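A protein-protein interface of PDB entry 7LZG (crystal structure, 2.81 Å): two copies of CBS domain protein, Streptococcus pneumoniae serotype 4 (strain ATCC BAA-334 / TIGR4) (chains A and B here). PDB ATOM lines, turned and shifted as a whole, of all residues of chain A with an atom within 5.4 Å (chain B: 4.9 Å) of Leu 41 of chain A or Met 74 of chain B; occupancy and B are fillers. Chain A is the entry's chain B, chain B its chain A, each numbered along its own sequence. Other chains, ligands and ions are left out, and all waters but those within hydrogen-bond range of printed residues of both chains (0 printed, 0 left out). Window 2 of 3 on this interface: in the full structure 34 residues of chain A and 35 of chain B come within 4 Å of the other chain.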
ATOM      1  N   ASP A  37      38.240  -0.142  27.696  1.00  0.00           N
ATOM      2  CA  ASP A  37      37.147   0.007  26.740  1.00  0.00           C
ATOM      3  C   ASP A  37      35.802  -0.287  27.392  1.00  0.00           C
ATOM      4  O   ASP A  37      34.861   0.510  27.284  1.00  0.00           O
ATOM      5  CB  ASP A  37      37.374  -0.904  25.534  1.00  0.00           C
ATOM      6  CG  ASP A  37      36.343  -0.691  24.443  1.00  0.00           C
ATOM      7  OD1 ASP A  37      36.381   0.376  23.793  1.00  0.00           O
ATOM      8  OD2 ASP A  37      35.496  -1.587  24.236  1.00  0.00           O
ATOM      9  N   HIS A  38      35.689  -1.428  28.076  1.00  0.00           N
ATOM     10  CA  HIS A  38      34.428  -1.772  28.724  1.00  0.00           C
ATOM     11  C   HIS A  38      34.182  -0.920  29.962  1.00  0.00           C
ATOM     12  O   HIS A  38      33.025  -0.715  30.352  1.00  0.00           O
ATOM     13  CB  HIS A  38      34.409  -3.259  29.083  1.00  0.00           C
ATOM     14  CG  HIS A  38      33.064  -3.762  29.505  1.00  0.00           C
ATOM     15  ND1 HIS A  38      32.725  -3.968  30.826  1.00  0.00           N
ATOM     16  CD2 HIS A  38      31.971  -4.101  28.781  1.00  0.00           C
ATOM     17  CE1 HIS A  38      31.483  -4.412  30.896  1.00  0.00           C
ATOM     18  NE2 HIS A  38      31.003  -4.501  29.668  1.00  0.00           N
ATOM     19  N   ALA A  39      35.247  -0.417  30.593  1.00  0.00           N
ATOM     20  CA  ALA A  39      35.074   0.479  31.731  1.00  0.00           C
ATOM     21  C   ALA A  39      34.402   1.782  31.318  1.00  0.00           C
ATOM     22  O   ALA A  39      33.674   2.381  32.117  1.00  0.00           O
ATOM     23  CB  ALA A  39      36.423   0.761  32.392  1.00  0.00           C
ATOM     24  N   THR A  40      34.631   2.234  30.083  1.00  0.00           N
ATOM     25  CA  THR A  40      33.933   3.417  29.590  1.00  0.00           C
ATOM     26  C   THR A  40      32.436   3.155  29.475  1.00  0.00           C
ATOM     27  O   THR A  40      31.616   3.985  29.883  1.00  0.00           O
ATOM     28  CB  THR A  40      34.510   3.853  28.243  1.00  0.00           C
ATOM     29  OG1 THR A  40      35.929   4.009  28.355  1.00  0.00           O
ATOM     30  CG2 THR A  40      33.902   5.176  27.810  1.00  0.00           C
ATOM     31  N   LEU A  41      32.060   2.001  28.915  1.00  0.00           N
ATOM     32  CA  LEU A  41      30.659   1.591  28.935  1.00  0.00           C
ATOM     33  C   LEU A  41      30.149   1.455  30.364  1.00  0.00           C
ATOM     34  O   LEU A  41      29.034   1.888  30.677  1.00  0.00           O
ATOM     35  CB  LEU A  41      30.485   0.271  28.183  1.00  0.00           C
ATOM     36  CG  LEU A  41      29.244  -0.563  28.517  1.00  0.00           C
ATOM     37  CD1 LEU A  41      27.964   0.134  28.082  1.00  0.00           C
ATOM     38  CD2 LEU A  41      29.343  -1.945  27.892  1.00  0.00           C
ATOM     39  N   LEU A  42      30.956   0.858  31.243  1.00  0.00           N
ATOM     40  CA  LEU A  42      30.536   0.665  32.627  1.00  0.00           C
ATOM     41  C   LEU A  42      30.351   2.000  33.340  1.00  0.00           C
ATOM     42  O   LEU A  42      29.374   2.188  34.073  1.00  0.00           O
ATOM     43  CB  LEU A  42      31.556  -0.208  33.357  1.00  0.00           C
ATOM     44  CG  LEU A  42      31.024  -1.409  34.143  1.00  0.00           C
ATOM     45  CD1 LEU A  42      29.801  -2.014  33.472  1.00  0.00           C
ATOM     46  CD2 LEU A  42      32.116  -2.455  34.283  1.00  0.00           C
ATOM     47  N   LEU A  43      31.273   2.942  33.130  1.00  0.00           N
ATOM     48  CA  LEU A  43      31.178   4.231  33.809  1.00  0.00           C
ATOM     49  C   LEU A  43      30.026   5.070  33.269  1.00  0.00           C
ATOM     50  O   LEU A  43      29.388   5.811  34.026  1.00  0.00           O
ATOM     51  CB  LEU A  43      32.497   4.992  33.678  1.00  0.00           C
ATOM     52  CG  LEU A  43      33.616   4.553  34.620  1.00  0.00           C
ATOM     53  CD1 LEU A  43      34.908   5.284  34.302  1.00  0.00           C
ATOM     54  CD2 LEU A  43      33.206   4.792  36.062  1.00  0.00           C
ATOM     55  N   SER A  44      29.743   4.968  31.967  1.00  0.00           N
ATOM     56  CA  SER A  44      28.680   5.776  31.379  1.00  0.00           C
ATOM     57  C   SER A  44      27.310   5.386  31.917  1.00  0.00           C
ATOM     58  O   SER A  44      26.394   6.217  31.935  1.00  0.00           O
ATOM     59  CB  SER A  44      28.701   5.651  29.857  1.00  0.00           C
ATOM     60  OG  SER A  44      28.261   4.370  29.445  1.00  0.00           O
ATOM     61  N   GLN A  45      27.149   4.139  32.359  1.00  0.00           N
ATOM     62  CA  GLN A  45      25.877   3.674  32.896  1.00  0.00           C
ATOM     63  C   GLN A  45      25.716   3.954  34.383  1.00  0.00           C
ATOM     64  O   GLN A  45      24.584   3.948  34.881  1.00  0.00           O
ATOM     65  CB  GLN A  45      25.716   2.174  32.639  1.00  0.00           C
ATOM     66  CG  GLN A  45      25.602   1.819  31.168  1.00  0.00           C
ATOM     67  CD  GLN A  45      24.492   2.586  30.477  1.00  0.00           C
ATOM     68  OE1 GLN A  45      23.309   2.364  30.741  1.00  0.00           O
ATOM     69  NE2 GLN A  45      24.869   3.503  29.593  1.00  0.00           N
ATOM     70  N   MET B  70      29.156  10.024  26.775  1.00  0.00           N
ATOM     71  CA  MET B  70      29.588   8.645  26.579  1.00  0.00           C
ATOM     72  C   MET B  70      28.412   7.684  26.675  1.00  0.00           C
ATOM     73  O   MET B  70      28.383   6.671  25.982  1.00  0.00           O
ATOM     74  CB  MET B  70      30.673   8.260  27.589  1.00  0.00           C
ATOM     75  CG  MET B  70      31.947   9.081  27.466  1.00  0.00           C
ATOM     76  SD  MET B  70      32.465   9.398  25.611  1.00  0.00           S
ATOM     77  CE  MET B  70      33.101   7.617  25.151  1.00  0.00           C
ATOM     78  N   ALA B  71      27.442   8.008  27.535  1.00  0.00           N
ATOM     79  CA  ALA B  71      26.243   7.181  27.626  1.00  0.00           C
ATOM     80  C   ALA B  71      25.479   7.186  26.313  1.00  0.00           C
ATOM     81  O   ALA B  71      25.044   6.133  25.835  1.00  0.00           O
ATOM     82  CB  ALA B  71      25.347   7.663  28.765  1.00  0.00           C
ATOM     83  N   TYR B  72      25.311   8.364  25.710  1.00  0.00           N
ATOM     84  CA  TYR B  72      24.662   8.440  24.407  1.00  0.00           C
ATOM     85  C   TYR B  72      25.440   7.651  23.360  1.00  0.00           C
ATOM     86  O   TYR B  72      24.849   6.920  22.557  1.00  0.00           O
ATOM     87  CB  TYR B  72      24.517   9.902  23.988  1.00  0.00           C
ATOM     88  CG  TYR B  72      23.804  10.101  22.674  1.00  0.00           C
ATOM     89  CD1 TYR B  72      22.422  10.211  22.622  1.00  0.00           C
ATOM     90  CD2 TYR B  72      24.514  10.181  21.485  1.00  0.00           C
ATOM     91  CE1 TYR B  72      21.768  10.393  21.421  1.00  0.00           C
ATOM     92  CE2 TYR B  72      23.868  10.362  20.282  1.00  0.00           C
ATOM     93  CZ  TYR B  72      22.497  10.467  20.254  1.00  0.00           C
ATOM     94  OH  TYR B  72      21.858  10.648  19.050  1.00  0.00           O
ATOM     95  N   GLN B  73      26.768   7.769  23.366  1.00  0.00           N
ATOM     96  CA  GLN B  73      27.573   7.077  22.366  1.00  0.00           C
ATOM     97  C   GLN B  73      27.610   5.574  22.608  1.00  0.00           C
ATOM     98  O   GLN B  73      27.741   4.799  21.655  1.00  0.00           O
ATOM     99  CB  GLN B  73      28.992   7.646  22.349  1.00  0.00           C
ATOM    100  CG  GLN B  73      29.850   7.126  21.208  1.00  0.00           C
ATOM    101  CD  GLN B  73      31.242   7.721  21.207  1.00  0.00           C
ATOM    102  OE1 GLN B  73      31.623   8.440  22.132  1.00  0.00           O
ATOM    103  NE2 GLN B  73      32.011   7.428  20.164  1.00  0.00           N
ATOM    104  N   MET B  74      27.490   5.143  23.859  1.00  0.00           N
ATOM    105  CA  MET B  74      27.593   3.726  24.187  1.00  0.00           C
ATOM    106  C   MET B  74      26.253   3.012  24.076  1.00  0.00           C
ATOM    107  O   MET B  74      26.164   1.936  23.485  1.00  0.00           O
ATOM    108  CB  MET B  74      28.154   3.544  25.595  1.00  0.00           C
ATOM    109  CG  MET B  74      29.228   2.481  25.689  1.00  0.00           C
ATOM    110  SD  MET B  74      30.852   3.025  24.774  1.00  0.00           S
ATOM    111  CE  MET B  74      31.050   4.768  25.609  1.00  0.00           C
ATOM    112  N   GLU B  75      25.214   3.613  24.665  1.00  0.00           N
ATOM    113  CA  GLU B  75      23.879   3.030  24.583  1.00  0.00           C
ATOM    114  C   GLU B  75      23.439   2.867  23.135  1.00  0.00           C
ATOM    115  O   GLU B  75      22.805   1.868  22.779  1.00  0.00           O
ATOM    116  CB  GLU B  75      22.875   3.895  25.344  1.00  0.00           C
ATOM    117  CG  GLU B  75      23.085   3.934  26.847  1.00  0.00           C
ATOM    118  CD  GLU B  75      22.261   5.016  27.517  1.00  0.00           C
ATOM    119  OE1 GLU B  75      21.486   5.696  26.810  1.00  0.00           O
ATOM    120  OE2 GLU B  75      22.393   5.190  28.747  1.00  0.00           O
ATOM    121  N   HIS B  76      23.770   3.837  22.286  1.00  0.00           N
ATOM    122  CA  HIS B  76      23.383   3.799  20.886  1.00  0.00           C
ATOM    123  C   HIS B  76      24.470   3.243  19.977  1.00  0.00           C
ATOM    124  O   HIS B  76      24.223   3.084  18.777  1.00  0.00           O
ATOM    125  CB  HIS B  76      22.982   5.199  20.412  1.00  0.00           C
ATOM    126  CG  HIS B  76      21.852   5.795  21.191  1.00  0.00           C
ATOM    127  ND1 HIS B  76      22.041   6.754  22.162  1.00  0.00           N
ATOM    128  CD2 HIS B  76      20.519   5.557  21.153  1.00  0.00           C
ATOM    129  CE1 HIS B  76      20.874   7.088  22.682  1.00  0.00           C
ATOM    130  NE2 HIS B  76      19.934   6.375  22.088  1.00  0.00           N
ATOM    131  N   ASP B  77      25.654   2.949  20.513  1.00  0.00           N
ATOM    132  CA  ASP B  77      26.739   2.314  19.765  1.00  0.00           C
ATOM    133  C   ASP B  77      27.025   3.070  18.466  1.00  0.00           C
ATOM    134  O   ASP B  77      26.894   2.543  17.360  1.00  0.00           O
ATOM    135  CB  ASP B  77      26.414   0.843  19.493  1.00  0.00           C
ATOM    136  CG  ASP B  77      27.562   0.096  18.842  1.00  0.00           C
ATOM    137  OD1 ASP B  77      28.718   0.564  18.942  1.00  0.00           O
ATOM    138  OD2 ASP B  77      27.305  -0.956  18.219  1.00  0.00           O
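The side-chain amide nitrogen (NE2) of Gln 45 of chain A is in hydrogen-bond range of the side-chain carboxylate (OE2) of Glu 75 of chain B.
The backbone carbonyl oxygen (O) of Leu 41 of chain A sits at hydrogen-bond distance from the side-chain hydroxyl (OG) of Ser 44 of chain A, at 2.9 Å.
The side-chain amide oxygen (OE1) of Gln 73 of chain B lies close to the side-chain sulfur (SD) of Met 70 of chain B, 3.7 Å away.
O of Thr 40 of chain A lies close to OG of Ser 44 of chain A (3.4 Å).
CE of Met 70 of chain B touches CG2 of Thr 40 of chain A, 3.7 Å away.
CE of Met 74 of chain B touches CG2 of Thr 40 of chain A, at 3.6 Å.
Met 74 of chain B touches Leu 41 of chain A.
Met 70 of chain B touches Ser 44 of chain A.
Ser 44 of chain A touches Ala 71 of chain B (CB to N, 3.5 Å).
OG of Ser 44 of chain A touches CB of Met 74 of chain B, 3.9 Å away.
Ala 39 of chain A touches none of the printed residues of chain B.
Of the printed residues of chain B, Thr 40 of chain A touches Met 70 and Met 74.
Of chain B, only Met 74 comes within 4 Å of Leu 41 of chain A.
Of the printed residues of chain B, Ser 44 of chain A touches Met 70, Ala 71 and Met 74.
Of the printed residues of chain A, Ala 71 of chain B touches Ser 44.
Printed residues of chain A within 4 Å of Glu 75 of chain B: Gln 45.
The nearest printed residue of chain B that does not touch Ser 44 of chain A is Glu 75 of chain B (5.2 Å).
Of the 9 printed residues of chain A, 4 touch a printed residue of chain B.
Printed residues of chain A that touch a printed residue of chain B: Thr 40, Leu 41, Ser 44 and Gln 45.
Along chain A the printed residues that touch a printed residue of chain B span positions 40 to 45.
Printed residues of chain B that touch a printed residue of chain A: Met 70, Ala 71, Met 74 and Glu 75.
Hydrophobic or aromatic side chains of chain B within 4 Å of the printed part of chain A: Met 70, Ala 71 and Met 74.
Among the printed residues, no Asp or Glu carboxylate lies within 4 Å of a Lys or Arg side-chain nitrogen of the other chain.
No position is printed for both chains.
Of the 7 pairs that touch across the chains among the printed residues, none has its exchanged pair printed and touching as well.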
